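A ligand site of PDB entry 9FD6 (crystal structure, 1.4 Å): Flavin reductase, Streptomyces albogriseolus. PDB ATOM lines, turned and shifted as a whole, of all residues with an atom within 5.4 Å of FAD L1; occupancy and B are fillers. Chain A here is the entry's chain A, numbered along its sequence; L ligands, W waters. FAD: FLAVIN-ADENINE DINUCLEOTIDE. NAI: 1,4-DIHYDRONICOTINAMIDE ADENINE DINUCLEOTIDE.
O of Gly 42 is in hydrogen-bond range of NH1 of Arg 101, at 3.0 Å.
OG1 of Thr 68 sits at hydrogen-bond distance from N of Met 43 (3.3 Å).
The side-chain hydroxyl (OG) of Ser 66 lies within hydrogen-bond range of the backbone NH (N) of Leu 69 (3.0 Å).
The guanidinium group (NH1) of Arg 101 sits at hydrogen-bond distance from the backbone carbonyl oxygen (O) of Phe 94.
OG1 of Thr 44 lies within hydrogen-bond range of O of Ala 91 (2.7 Å).
O of Arg 63 sits at hydrogen-bond distance from OG of Ser 66, at 2.8 Å.
O of Asp 98 sits at hydrogen-bond distance from NE of Arg 101.
The backbone NH of Thr 44 lies within hydrogen-bond range of the backbone carbonyl oxygen of Phe 94 (2.9 Å).
A nitrogen (N1) of FAD L1 lies within hydrogen-bond range of a nitrogen (N7N) of NAI L2 (3.3 Å).
Water W3 lies within hydrogen-bond range of an oxygen (O3') of FAD L1 and the guanidinium group (NH1) of Arg 63.
Water W4 lies within hydrogen-bond range of O2A of FAD L1 (2.6 Å) and O of Gly 65 (2.9 Å).
Water W6 bridges O4' of FAD L1 (2.8 Å) and O of Gly 96 (3.3 Å).
Water W2 lies within hydrogen-bond range of an oxygen (O1P) of FAD L1 and the backbone NH (N) of Gly 42.
The backbone NH of Thr 44 lies within hydrogen-bond range of an oxygen (O2') of FAD L1 (3.4 Å).
O2N of NAI L2 lies within hydrogen-bond range of OH of Tyr 158, at 2.6 Å.
N of Ala 67 lies within hydrogen-bond range of O2A of FAD L1.
An oxygen (O4) of FAD L1 is in hydrogen-bond range of the backbone NH of Ser 47 (3.3 Å).
The guanidinium group (NH1) of Arg 101 is in salt-bridge range of an oxygen (O1P) of FAD L1 (3.3 Å).
The side-chain sulfur of Cys 45 is in hydrogen-bond range of an oxygen (O4) of FAD L1 (3.5 Å).
OG1 of Thr 68 is in hydrogen-bond range of O2P of FAD L1.
The backbone NH of Arg 63 sits at hydrogen-bond distance from an oxygen (O2) of FAD L1 (2.9 Å).
A nitrogen (N7N) of NAI L2 lies within hydrogen-bond range of a ring nitrogen (NE2) of His 138.
The backbone NH (N) of Thr 68 sits at hydrogen-bond distance from an oxygen (O2P) of FAD L1, at 2.9 Å.
O of Pro 97 lies within hydrogen-bond range of O3B of FAD L1.
O of Gly 96 lies within hydrogen-bond range of O4' of FAD L1, 3.2 Å away.
The backbone carbonyl oxygen (O) of Thr 44 lies within hydrogen-bond range of an oxygen (O2') of FAD L1 (2.8 Å).
An oxygen (O2') of FAD L1 sits close to the backbone carbonyl oxygen of Phe 94 (3.4 Å).
A nitrogen (N5) of FAD L1 sits at hydrogen-bond distance from the backbone NH (N) of Ser 46 (3.2 Å).
An oxygen (O4) of FAD L1 sits at hydrogen-bond distance from the side-chain hydroxyl (OG) of Ser 47 (2.8 Å).
The backbone carbonyl oxygen of Cys 61 is in hydrogen-bond range of a nitrogen (N3) of FAD L1.
The guanidinium group (NH2) of Arg 63 lies within salt-bridge range of an oxygen (O1A) of FAD L1, at 2.7 Å.
A nitrogen (N5) of FAD L1 sits at hydrogen-bond distance from the side-chain hydroxyl (OG) of Ser 46 (3.2 Å).
NH2 of Arg 41 lies close to N6A of FAD L1 (3.3 Å).
O2 of FAD L1 lies close to SD of Met 43 (3.3 Å).
Merely in contact with FAD L1: Leu 62 (3.4 Å), Ser 95 (3.4 Å), Ser 66 (3.4 Å), Pro 99 (3.5 Å), Gly 42 (3.6 Å), Tyr 158 (3.6 Å), Ile 28 (3.7 Å) and His 138 (3.9 Å).
Within 4 Å of FAD L1: Ile 28, Arg 41, Gly 42, Met 43, Thr 44, Cys 45, Ser 46, Ser 47, Cys 61, Leu 62, Arg 63, Ser 66, Ala 67, Thr 68, Phe 94, Ser 95, Gly 96, Pro 97, Pro 99, Arg 101, His 138 and Tyr 158.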
ATOM      1  N   ILE A  28       8.403  17.498 -24.390  1.00  0.00           N
ATOM      2  CA  ILE A  28       7.431  18.305 -23.663  1.00  0.00           C
ATOM      3  C   ILE A  28       7.894  18.421 -22.217  1.00  0.00           C
ATOM      4  O   ILE A  28       8.166  17.404 -21.575  1.00  0.00           O
ATOM      5  CB  ILE A  28       6.021  17.712 -23.721  1.00  0.00           C
ATOM      6  CG1 ILE A  28       5.428  17.879 -25.113  1.00  0.00           C
ATOM      7  CG2 ILE A  28       5.140  18.387 -22.684  1.00  0.00           C
ATOM      8  CD1 ILE A  28       5.068  19.307 -25.491  1.00  0.00           C
ATOM      9  N   ASP A  35       4.702  31.598  -7.101  1.00  0.00           N
ATOM     10  CA  ASP A  35       4.428  33.032  -7.190  1.00  0.00           C
ATOM     11  C   ASP A  35       4.896  33.735  -5.907  1.00  0.00           C
ATOM     12  O   ASP A  35       5.468  33.119  -5.007  1.00  0.00           O
ATOM     13  CB  ASP A  35       2.987  33.330  -7.607  1.00  0.00           C
ATOM     14  CG  ASP A  35       1.968  33.117  -6.518  1.00  0.00           C
ATOM     15  OD1 ASP A  35       2.342  32.899  -5.344  1.00  0.00           O
ATOM     16  OD2 ASP A  35       0.767  33.153  -6.862  1.00  0.00           O
ATOM     17  N   ARG A  41       2.882  27.546  -9.587  1.00  0.00           N
ATOM     18  CA  ARG A  41       2.402  27.891 -10.901  1.00  0.00           C
ATOM     19  C   ARG A  41       3.197  27.076 -11.914  1.00  0.00           C
ATOM     20  O   ARG A  41       4.351  26.716 -11.664  1.00  0.00           O
ATOM     21  CB  ARG A  41       2.590  29.384 -11.200  1.00  0.00           C
ATOM     22  CG  ARG A  41       1.874  30.319 -10.235  1.00  0.00           C
ATOM     23  CD  ARG A  41       0.337  30.170 -10.201  1.00  0.00           C
ATOM     24  NE  ARG A  41      -0.222  31.085  -9.201  1.00  0.00           N
ATOM     25  CZ  ARG A  41      -1.468  31.053  -8.762  1.00  0.00           C
ATOM     26  NH1 ARG A  41      -2.363  30.206  -9.262  1.00  0.00           N
ATOM     27  NH2 ARG A  41      -1.842  31.896  -7.797  1.00  0.00           N
ATOM     28  N   GLY A  42       2.581  26.763 -13.039  1.00  0.00           N
ATOM     29  CA  GLY A  42       3.310  26.039 -14.069  1.00  0.00           C
ATOM     30  C   GLY A  42       2.544  25.986 -15.370  1.00  0.00           C
ATOM     31  O   GLY A  42       1.344  26.273 -15.426  1.00  0.00           O
ATOM     32  N   MET A  43       3.269  25.624 -16.420  1.00  0.00           N
ATOM     33  CA  MET A  43       2.679  25.488 -17.735  1.00  0.00           C
ATOM     34  C   MET A  43       3.426  24.450 -18.562  1.00  0.00           C
ATOM     35  O   MET A  43       4.636  24.231 -18.393  1.00  0.00           O
ATOM     36  CB  MET A  43       2.694  26.822 -18.520  1.00  0.00           C
ATOM     37  CG  MET A  43       4.078  27.274 -19.008  1.00  0.00           C
ATOM     38  SD  MET A  43       4.012  28.428 -20.405  1.00  0.00           S
ATOM     39  CE  MET A  43       3.466  29.937 -19.609  1.00  0.00           C
ATOM     40  N   THR A  44       2.702  23.851 -19.485  1.00  0.00           N
ATOM     41  CA  THR A  44       3.299  23.009 -20.500  1.00  0.00           C
ATOM     42  C   THR A  44       4.156  23.869 -21.419  1.00  0.00           C
ATOM     43  O   THR A  44       3.735  24.952 -21.837  1.00  0.00           O
ATOM     44  CB  THR A  44       2.178  22.318 -21.268  1.00  0.00           C
ATOM     45  OG1 THR A  44       1.456  21.496 -20.350  1.00  0.00           O
ATOM     46  CG2 THR A  44       2.727  21.448 -22.370  1.00  0.00           C
ATOM     47  N   CYS A  45       5.362  23.395 -21.702  1.00  0.00           N
ATOM     48  CA  CYS A  45       6.360  24.172 -22.421  1.00  0.00           C
ATOM     49  C   CYS A  45       7.058  23.273 -23.417  1.00  0.00           C
ATOM     50  O   CYS A  45       7.604  22.232 -23.043  1.00  0.00           O
ATOM     51  CB  CYS A  45       7.364  24.746 -21.419  1.00  0.00           C
ATOM     52  SG  CYS A  45       8.644  25.702 -22.144  1.00  0.00           S
ATOM     53  N   SER A  46       7.034  23.684 -24.677  1.00  0.00           N
ATOM     54  CA  SER A  46       7.742  23.012 -25.750  1.00  0.00           C
ATOM     55  C   SER A  46       8.954  23.807 -26.227  1.00  0.00           C
ATOM     56  O   SER A  46       9.634  23.367 -27.155  1.00  0.00           O
ATOM     57  CB  SER A  46       6.790  22.761 -26.929  1.00  0.00           C
ATOM     58  OG  SER A  46       6.222  23.974 -27.392  1.00  0.00           O
ATOM     59  N   SER A  47       9.253  24.941 -25.605  1.00  0.00           N
ATOM     60  CA  SER A  47      10.304  25.845 -26.072  1.00  0.00           C
ATOM     61  C   SER A  47      11.630  25.658 -25.335  1.00  0.00           C
ATOM     62  O   SER A  47      12.488  26.548 -25.376  1.00  0.00           O
ATOM     63  CB  SER A  47       9.827  27.296 -25.981  1.00  0.00           C
ATOM     64  OG  SER A  47       9.391  27.599 -24.655  1.00  0.00           O
ATOM     65  N   CYS A  61      10.675  29.941 -23.529  1.00  0.00           N
ATOM     66  CA  CYS A  61       9.962  31.111 -24.027  1.00  0.00           C
ATOM     67  C   CYS A  61       8.546  31.079 -23.468  1.00  0.00           C
ATOM     68  O   CYS A  61       7.761  30.194 -23.833  1.00  0.00           O
ATOM     69  CB  CYS A  61       9.970  31.137 -25.554  1.00  0.00           C
ATOM     70  SG  CYS A  61       9.287  32.642 -26.239  1.00  0.00           S
ATOM     71  N   LEU A  62       8.221  32.035 -22.600  1.00  0.00           N
ATOM     72  CA  LEU A  62       6.960  32.063 -21.876  1.00  0.00           C
ATOM     73  C   LEU A  62       6.120  33.281 -22.222  1.00  0.00           C
ATOM     74  O   LEU A  62       6.643  34.386 -22.387  1.00  0.00           O
ATOM     75  CB  LEU A  62       7.221  32.064 -20.364  1.00  0.00           C
ATOM     76  CG  LEU A  62       8.128  30.952 -19.825  1.00  0.00           C
ATOM     77  CD1 LEU A  62       8.340  31.171 -18.338  1.00  0.00           C
ATOM     78  CD2 LEU A  62       7.566  29.560 -20.078  1.00  0.00           C
ATOM     79  N   ARG A  63       4.812  33.083 -22.302  1.00  0.00           N
ATOM     80  CA  ARG A  63       3.897  34.147 -22.675  1.00  0.00           C
ATOM     81  C   ARG A  63       3.843  35.253 -21.624  1.00  0.00           C
ATOM     82  O   ARG A  63       3.739  34.992 -20.423  1.00  0.00           O
ATOM     83  CB  ARG A  63       2.495  33.555 -22.862  1.00  0.00           C
ATOM     84  CG  ARG A  63       1.491  34.523 -23.440  1.00  0.00           C
ATOM     85  CD  ARG A  63       0.095  33.922 -23.400  1.00  0.00           C
ATOM     86  NE  ARG A  63      -0.588  34.294 -22.172  1.00  0.00           N
ATOM     87  CZ  ARG A  63      -1.061  33.443 -21.252  1.00  0.00           C
ATOM     88  NH1 ARG A  63      -0.986  32.132 -21.428  1.00  0.00           N
ATOM     89  NH2 ARG A  63      -1.634  33.928 -20.166  1.00  0.00           N
ATOM     90  N   GLY A  65       2.328  37.934 -19.247  1.00  0.00           N
ATOM     91  CA  GLY A  65       1.077  37.906 -18.516  1.00  0.00           C
ATOM     92  C   GLY A  65       0.667  36.540 -18.011  1.00  0.00           C
ATOM     93  O   GLY A  65      -0.330  36.448 -17.288  1.00  0.00           O
ATOM     94  N   SER A  66       1.386  35.476 -18.371  1.00  0.00           N
ATOM     95  CA  SER A  66       1.057  34.166 -17.850  1.00  0.00           C
ATOM     96  C   SER A  66       1.395  34.075 -16.371  1.00  0.00           C
ATOM     97  O   SER A  66       2.327  34.719 -15.871  1.00  0.00           O
ATOM     98  CB  SER A  66       1.815  33.072 -18.605  1.00  0.00           C
ATOM     99  OG  SER A  66       3.221  33.127 -18.386  1.00  0.00           O
ATOM    100  N   ALA A  67       0.616  33.266 -15.663  1.00  0.00           N
ATOM    101  CA  ALA A  67       0.876  33.031 -14.245  1.00  0.00           C
ATOM    102  C   ALA A  67       2.278  32.475 -14.052  1.00  0.00           C
ATOM    103  O   ALA A  67       2.982  32.843 -13.102  1.00  0.00           O
ATOM    104  CB  ALA A  67      -0.177  32.094 -13.675  1.00  0.00           C
ATOM    105  N   THR A  68       2.721  31.594 -14.952  1.00  0.00           N
ATOM    106  CA  THR A  68       4.039  30.990 -14.782  1.00  0.00           C
ATOM    107  C   THR A  68       5.132  32.035 -14.945  1.00  0.00           C
ATOM    108  O   THR A  68       6.059  32.102 -14.125  1.00  0.00           O
ATOM    109  CB  THR A  68       4.225  29.835 -15.764  1.00  0.00           C
ATOM    110  OG1 THR A  68       3.241  28.816 -15.532  1.00  0.00           O
ATOM    111  CG2 THR A  68       5.603  29.235 -15.603  1.00  0.00           C
ATOM    112  N   LEU A  69       5.068  32.863 -15.990  1.00  0.00           N
ATOM    113  CA  LEU A  69       6.105  33.878 -16.161  1.00  0.00           C
ATOM    114  C   LEU A  69       6.119  34.846 -14.991  1.00  0.00           C
ATOM    115  O   LEU A  69       7.190  35.266 -14.540  1.00  0.00           O
ATOM    116  CB  LEU A  69       5.937  34.637 -17.473  1.00  0.00           C
ATOM    117  CG  LEU A  69       6.966  35.753 -17.662  1.00  0.00           C
ATOM    118  CD1 LEU A  69       8.386  35.189 -17.641  1.00  0.00           C
ATOM    119  CD2 LEU A  69       6.724  36.534 -18.962  1.00  0.00           C
ATOM    120  N   ALA A  91       0.463  17.087 -19.396  1.00  0.00           N
ATOM    121  CA  ALA A  91       0.683  18.092 -20.420  1.00  0.00           C
ATOM    122  C   ALA A  91      -0.621  18.767 -20.825  1.00  0.00           C
ATOM    123  O   ALA A  91      -0.655  19.972 -21.088  1.00  0.00           O
ATOM    124  CB  ALA A  91       1.340  17.464 -21.651  1.00  0.00           C
ATOM    125  N   PHE A  94      -1.765  21.075 -17.859  1.00  0.00           N
ATOM    126  CA  PHE A  94      -0.902  22.243 -17.724  1.00  0.00           C
ATOM    127  C   PHE A  94      -0.867  23.124 -18.967  1.00  0.00           C
ATOM    128  O   PHE A  94      -0.162  24.135 -18.970  1.00  0.00           O
ATOM    129  CB  PHE A  94       0.492  21.811 -17.284  1.00  0.00           C
ATOM    130  CG  PHE A  94       0.609  21.647 -15.811  1.00  0.00           C
ATOM    131  CD1 PHE A  94       0.164  20.488 -15.207  1.00  0.00           C
ATOM    132  CD2 PHE A  94       1.094  22.665 -15.023  1.00  0.00           C
ATOM    133  CE1 PHE A  94       0.225  20.338 -13.830  1.00  0.00           C
ATOM    134  CE2 PHE A  94       1.176  22.512 -13.640  1.00  0.00           C
ATOM    135  CZ  PHE A  94       0.742  21.350 -13.058  1.00  0.00           C
ATOM    136  N   SER A  95      -1.629  22.785 -20.012  1.00  0.00           N
ATOM    137  CA  SER A  95      -1.806  23.675 -21.147  1.00  0.00           C
ATOM    138  C   SER A  95      -3.230  24.191 -21.272  1.00  0.00           C
ATOM    139  O   SER A  95      -3.548  24.915 -22.226  1.00  0.00           O
ATOM    140  CB  SER A  95      -1.429  22.954 -22.441  1.00  0.00           C
ATOM    141  OG  SER A  95      -2.273  21.841 -22.657  1.00  0.00           O
ATOM    142  N   GLY A  96      -4.100  23.810 -20.340  1.00  0.00           N
ATOM    143  CA  GLY A  96      -5.499  24.131 -20.421  1.00  0.00           C
ATOM    144  C   GLY A  96      -5.888  25.331 -19.577  1.00  0.00           C
ATOM    145  O   GLY A  96      -5.035  26.076 -19.078  1.00  0.00           O
ATOM    146  N   PRO A  97      -7.191  25.541 -19.416  1.00  0.00           N
ATOM    147  CA  PRO A  97      -7.688  26.757 -18.765  1.00  0.00           C
ATOM    148  C   PRO A  97      -7.811  26.690 -17.246  1.00  0.00           C
ATOM    149  O   PRO A  97      -8.153  27.714 -16.641  1.00  0.00           O
ATOM    150  CB  PRO A  97      -9.093  26.887 -19.378  1.00  0.00           C
ATOM    151  CG  PRO A  97      -9.531  25.491 -19.586  1.00  0.00           C
ATOM    152  CD  PRO A  97      -8.272  24.754 -20.025  1.00  0.00           C
ATOM    153  N   ASP A  98      -7.527  25.548 -16.630  1.00  0.00           N
ATOM    154  CA  ASP A  98      -7.863  25.348 -15.223  1.00  0.00           C
ATOM    155  C   ASP A  98      -6.698  25.805 -14.352  1.00  0.00           C
ATOM    156  O   ASP A  98      -5.621  25.214 -14.428  1.00  0.00           O
ATOM    157  CB  ASP A  98      -8.148  23.880 -14.983  1.00  0.00           C
ATOM    158  CG  ASP A  98      -8.663  23.607 -13.591  1.00  0.00           C
ATOM    159  OD1 ASP A  98      -8.723  24.549 -12.769  1.00  0.00           O
ATOM    160  OD2 ASP A  98      -9.009  22.423 -13.341  1.00  0.00           O
ATOM    161  N   PRO A  99      -6.877  26.848 -13.524  1.00  0.00           N
ATOM    162  CA  PRO A  99      -5.773  27.248 -12.627  1.00  0.00           C
ATOM    163  C   PRO A  99      -5.495  26.242 -11.529  1.00  0.00           C
ATOM    164  O   PRO A  99      -4.429  26.312 -10.913  1.00  0.00           O
ATOM    165  CB  PRO A  99      -6.270  28.571 -12.037  1.00  0.00           C
ATOM    166  CG  PRO A  99      -7.749  28.437 -12.047  1.00  0.00           C
ATOM    167  CD  PRO A  99      -8.076  27.678 -13.320  1.00  0.00           C
ATOM    168  N   ARG A 101      -4.652  23.276 -11.776  1.00  0.00           N
ATOM    169  CA  ARG A 101      -3.852  22.192 -12.354  1.00  0.00           C
ATOM    170  C   ARG A 101      -3.063  21.392 -11.332  1.00  0.00           C
ATOM    171  O   ARG A 101      -2.901  20.172 -11.480  1.00  0.00           O
ATOM    172  CB  ARG A 101      -2.921  22.792 -13.416  1.00  0.00           C
ATOM    173  CG  ARG A 101      -2.049  23.951 -12.912  1.00  0.00           C
ATOM    174  CD  ARG A 101      -1.553  24.822 -14.052  1.00  0.00           C
ATOM    175  NE  ARG A 101      -2.658  25.301 -14.867  1.00  0.00           N
ATOM    176  CZ  ARG A 101      -2.519  25.766 -16.099  1.00  0.00           C
ATOM    177  NH1 ARG A 101      -1.334  25.901 -16.654  1.00  0.00           N
ATOM    178  NH2 ARG A 101      -3.602  26.076 -16.790  1.00  0.00           N
ATOM    179  N   HIS A 138       6.020  37.577 -25.744  1.00  0.00           N
ATOM    180  CA  HIS A 138       6.666  36.521 -24.998  1.00  0.00           C
ATOM    181  C   HIS A 138       7.945  37.047 -24.387  1.00  0.00           C
ATOM    182  O   HIS A 138       8.440  38.123 -24.738  1.00  0.00           O
ATOM    183  CB  HIS A 138       7.003  35.325 -25.890  1.00  0.00           C
ATOM    184  CG  HIS A 138       5.864  34.390 -26.092  1.00  0.00           C
ATOM    185  ND1 HIS A 138       4.690  34.762 -26.702  1.00  0.00           N
ATOM    186  CD2 HIS A 138       5.712  33.093 -25.753  1.00  0.00           C
ATOM    187  CE1 HIS A 138       3.864  33.741 -26.732  1.00  0.00           C
ATOM    188  NE2 HIS A 138       4.462  32.710 -26.166  1.00  0.00           N
ATOM    189  N   TYR A 158       5.675  16.031 -28.854  1.00  0.00           N
ATOM    190  CA  TYR A 158       4.537  16.724 -29.434  1.00  0.00           C
ATOM    191  C   TYR A 158       4.973  17.282 -30.780  1.00  0.00           C
ATOM    192  O   TYR A 158       6.027  17.916 -30.876  1.00  0.00           O
ATOM    193  CB  TYR A 158       4.059  17.859 -28.536  1.00  0.00           C
ATOM    194  CG  TYR A 158       2.698  18.398 -28.916  1.00  0.00           C
ATOM    195  CD1 TYR A 158       1.545  17.787 -28.452  1.00  0.00           C
ATOM    196  CD2 TYR A 158       2.569  19.509 -29.733  1.00  0.00           C
ATOM    197  CE1 TYR A 158       0.293  18.283 -28.785  1.00  0.00           C
ATOM    198  CE2 TYR A 158       1.316  20.012 -30.071  1.00  0.00           C
ATOM    199  CZ  TYR A 158       0.184  19.395 -29.587  1.00  0.00           C
ATOM    200  OH  TYR A 158      -1.074  19.875 -29.921  1.00  0.00           O
ATOM    201  N   PHE A 163       0.334  14.383 -29.708  1.00  0.00           N
ATOM    202  CA  PHE A 163       1.259  13.721 -28.819  1.00  0.00           C
ATOM    203  C   PHE A 163       1.732  12.411 -29.436  1.00  0.00           C
ATOM    204  O   PHE A 163       1.002  11.749 -30.180  1.00  0.00           O
ATOM    205  CB  PHE A 163       0.607  13.413 -27.468  1.00  0.00           C
ATOM    206  CG  PHE A 163       0.366  14.633 -26.634  1.00  0.00           C
ATOM    207  CD1 PHE A 163       1.382  15.175 -25.863  1.00  0.00           C
ATOM    208  CD2 PHE A 163      -0.869  15.248 -26.635  1.00  0.00           C
ATOM    209  CE1 PHE A 163       1.156  16.305 -25.109  1.00  0.00           C
ATOM    210  CE2 PHE A 163      -1.094  16.371 -25.889  1.00  0.00           C
ATOM    211  CZ  PHE A 163      -0.097  16.903 -25.125  1.00  0.00           C
HETATM  212  PA  FAD L   1      -2.292  31.590 -17.574  1.00  0.00           P
HETATM  213  O1A FAD L   1      -2.841  31.793 -18.963  1.00  0.00           O
HETATM  214  O2A FAD L   1      -1.850  32.741 -16.743  1.00  0.00           O
HETATM  215  O5B FAD L   1      -3.377  30.747 -16.709  1.00  0.00           O
HETATM  216  C5B FAD L   1      -4.104  29.638 -17.185  1.00  0.00           C
HETATM  217  C4B FAD L   1      -5.526  29.755 -16.603  1.00  0.00           C
HETATM  218  O4B FAD L   1      -5.478  30.033 -15.197  1.00  0.00           O
HETATM  219  C3B FAD L   1      -6.327  30.894 -17.228  1.00  0.00           C
HETATM  220  O3B FAD L   1      -7.680  30.502 -17.248  1.00  0.00           O
HETATM  221  C2B FAD L   1      -6.062  32.027 -16.250  1.00  0.00           C
HETATM  222  O2B FAD L   1      -7.050  33.018 -16.329  1.00  0.00           O
HETATM  223  C1B FAD L   1      -6.022  31.306 -14.894  1.00  0.00           C
HETATM  224  N9A FAD L   1      -5.211  31.938 -13.872  1.00  0.00           N
HETATM  225  C8A FAD L   1      -3.914  32.345 -14.013  1.00  0.00           C
HETATM  226  N7A FAD L   1      -3.407  32.867 -12.927  1.00  0.00           N
HETATM  227  C5A FAD L   1      -4.425  32.801 -12.008  1.00  0.00           C
HETATM  228  C6A FAD L   1      -4.502  33.209 -10.671  1.00  0.00           C
HETATM  229  N6A FAD L   1      -3.472  33.768 -10.026  1.00  0.00           N
HETATM  230  N1A FAD L   1      -5.661  32.990 -10.032  1.00  0.00           N
HETATM  231  C2A FAD L   1      -6.670  32.422 -10.693  1.00  0.00           C
HETATM  232  N3A FAD L   1      -6.712  32.015 -11.955  1.00  0.00           N
HETATM  233  C4A FAD L   1      -5.562  32.223 -12.573  1.00  0.00           C
HETATM  234  N1  FAD L   1       3.134  28.462 -23.669  1.00  0.00           N
HETATM  235  C2  FAD L   1       4.289  29.183 -23.539  1.00  0.00           C
HETATM  236  O2  FAD L   1       4.322  30.309 -23.073  1.00  0.00           O
HETATM  237  N3  FAD L   1       5.472  28.590 -23.961  1.00  0.00           N
HETATM  238  C4  FAD L   1       5.621  27.339 -24.511  1.00  0.00           C
HETATM  239  O4  FAD L   1       6.691  26.883 -24.850  1.00  0.00           O
HETATM  240  C4X FAD L   1       4.352  26.576 -24.648  1.00  0.00           C
HETATM  241  N5  FAD L   1       4.391  25.375 -25.160  1.00  0.00           N
HETATM  242  C5X FAD L   1       3.223  24.672 -25.281  1.00  0.00           C
HETATM  243  C6  FAD L   1       3.219  23.367 -25.844  1.00  0.00           C
HETATM  244  C7  FAD L   1       2.079  22.621 -25.992  1.00  0.00           C
HETATM  245  C7M FAD L   1       2.086  21.249 -26.591  1.00  0.00           C
HETATM  246  C8  FAD L   1       0.864  23.217 -25.576  1.00  0.00           C
HETATM  247  C8M FAD L   1      -0.442  22.489 -25.694  1.00  0.00           C
HETATM  248  C9  FAD L   1       0.844  24.482 -25.022  1.00  0.00           C
HETATM  249  C9A FAD L   1       2.002  25.251 -24.852  1.00  0.00           C
HETATM  250  N10 FAD L   1       1.999  26.535 -24.311  1.00  0.00           N
HETATM  251  C10 FAD L   1       3.156  27.243 -24.183  1.00  0.00           C
HETATM  252  C1' FAD L   1       0.761  27.161 -23.807  1.00  0.00           C
HETATM  253  C2' FAD L   1       0.715  27.003 -22.256  1.00  0.00           C
HETATM  254  O2' FAD L   1       1.016  25.687 -21.808  1.00  0.00           O
HETATM  255  C3' FAD L   1      -0.672  27.386 -21.678  1.00  0.00           C
HETATM  256  O3' FAD L   1      -0.952  28.702 -22.098  1.00  0.00           O
HETATM  257  C4' FAD L   1      -0.743  27.253 -20.138  1.00  0.00           C
HETATM  258  O4' FAD L   1      -2.097  27.022 -19.771  1.00  0.00           O
HETATM  259  C5' FAD L   1      -0.193  28.477 -19.403  1.00  0.00           C
HETATM  260  O5' FAD L   1      -0.358  28.287 -18.022  1.00  0.00           O
HETATM  261  P   FAD L   1      -0.186  29.500 -16.926  1.00  0.00           P
HETATM  262  O1P FAD L   1      -0.908  29.057 -15.707  1.00  0.00           O
HETATM  263  O2P FAD L   1       1.218  30.008 -16.891  1.00  0.00           O
HETATM  264  O3P FAD L   1      -0.958  30.687 -17.755  1.00  0.00           O
HETATM  265  PA  NAI L   2      -0.988  25.415 -33.503  1.00  0.00           P
HETATM  266  O1A NAI L   2      -1.170  25.258 -34.970  1.00  0.00           O
HETATM  267  O2A NAI L   2      -1.867  26.333 -32.712  1.00  0.00           O
HETATM  268  O5B NAI L   2       0.546  25.903 -33.204  1.00  0.00           O
HETATM  269  C5B NAI L   2       1.582  25.358 -33.978  1.00  0.00           C
HETATM  270  C4B NAI L   2       2.930  25.830 -33.495  1.00  0.00           C
HETATM  271  O4B NAI L   2       3.053  27.243 -33.686  1.00  0.00           O
HETATM  272  C3B NAI L   2       3.145  25.631 -32.009  1.00  0.00           C
HETATM  273  O3B NAI L   2       3.544  24.310 -31.763  1.00  0.00           O
HETATM  274  C2B NAI L   2       4.269  26.650 -31.812  1.00  0.00           C
HETATM  275  O2B NAI L   2       5.502  26.176 -32.259  1.00  0.00           O
HETATM  276  C1B NAI L   2       3.781  27.830 -32.651  1.00  0.00           C
HETATM  277  N9A NAI L   2       2.964  28.746 -31.876  1.00  0.00           N
HETATM  278  C8A NAI L   2       1.606  28.688 -31.727  1.00  0.00           C
HETATM  279  N7A NAI L   2       1.122  29.612 -30.956  1.00  0.00           N
HETATM  280  C5A NAI L   2       2.200  30.336 -30.567  1.00  0.00           C
HETATM  281  C6A NAI L   2       2.322  31.460 -29.741  1.00  0.00           C
HETATM  282  N6A NAI L   2       1.274  32.047 -29.168  1.00  0.00           N
HETATM  283  N1A NAI L   2       3.537  31.961 -29.543  1.00  0.00           N
HETATM  284  C2A NAI L   2       4.567  31.359 -30.130  1.00  0.00           C
HETATM  285  N3A NAI L   2       4.586  30.299 -30.926  1.00  0.00           N
HETATM  286  C4A NAI L   2       3.359  29.810 -31.123  1.00  0.00           C
HETATM  287  O3  NAI L   2      -1.007  23.916 -32.870  1.00  0.00           O
HETATM  288  PN  NAI L   2      -0.299  23.203 -31.580  1.00  0.00           P
HETATM  289  O1N NAI L   2       1.166  23.044 -31.826  1.00  0.00           O
HETATM  290  O2N NAI L   2      -1.186  22.037 -31.294  1.00  0.00           O
HETATM  291  O5D NAI L   2      -0.421  24.309 -30.370  1.00  0.00           O
HETATM  292  C5D NAI L   2      -1.686  24.512 -29.799  1.00  0.00           C
HETATM  293  C4D NAI L   2      -1.663  25.743 -28.917  1.00  0.00           C
HETATM  294  O4D NAI L   2      -0.725  25.662 -27.835  1.00  0.00           O
HETATM  295  C3D NAI L   2      -1.237  26.989 -29.696  1.00  0.00           C
HETATM  296  O3D NAI L   2      -2.333  27.489 -30.425  1.00  0.00           O
HETATM  297  C2D NAI L   2      -0.867  27.895 -28.510  1.00  0.00           C
HETATM  298  O2D NAI L   2      -1.963  28.480 -27.865  1.00  0.00           O
HETATM  299  C1D NAI L   2      -0.179  26.917 -27.551  1.00  0.00           C
HETATM  300  N1N NAI L   2       1.256  26.943 -27.679  1.00  0.00           N
HETATM  301  C2N NAI L   2       1.966  28.028 -27.290  1.00  0.00           C
HETATM  302  C3N NAI L   2       3.294  28.193 -27.478  1.00  0.00           C
HETATM  303  C7N NAI L   2       3.926  29.438 -27.021  1.00  0.00           C
HETATM  304  O7N NAI L   2       5.129  29.686 -27.174  1.00  0.00           O
HETATM  305  N7N NAI L   2       3.093  30.310 -26.406  1.00  0.00           N
HETATM  306  C4N NAI L   2       4.147  27.096 -28.051  1.00  0.00           C
HETATM  307  C5N NAI L   2       3.260  25.973 -28.509  1.00  0.00           C
HETATM  308  C6N NAI L   2       1.972  25.877 -28.230  1.00  0.00           C
HETATM  309  O   HOH W   1      -9.504  32.260 -15.663  1.00  0.00           O
HETATM  310  O   HOH W   2      -0.002  28.146 -13.243  1.00  0.00           O
HETATM  311  O   HOH W   3       0.906  30.364 -22.739  1.00  0.00           O
HETATM  312  O   HOH W   4      -2.437  35.127 -15.844  1.00  0.00           O
HETATM  313  O   HOH W   5      -2.525  28.581 -24.294  1.00  0.00           O
HETATM  314  O   HOH W   6      -4.070  28.659 -20.825  1.00  0.00           O
HETATM  315  O   HOH W   7      -3.115  29.371 -13.990  1.00  0.00           O
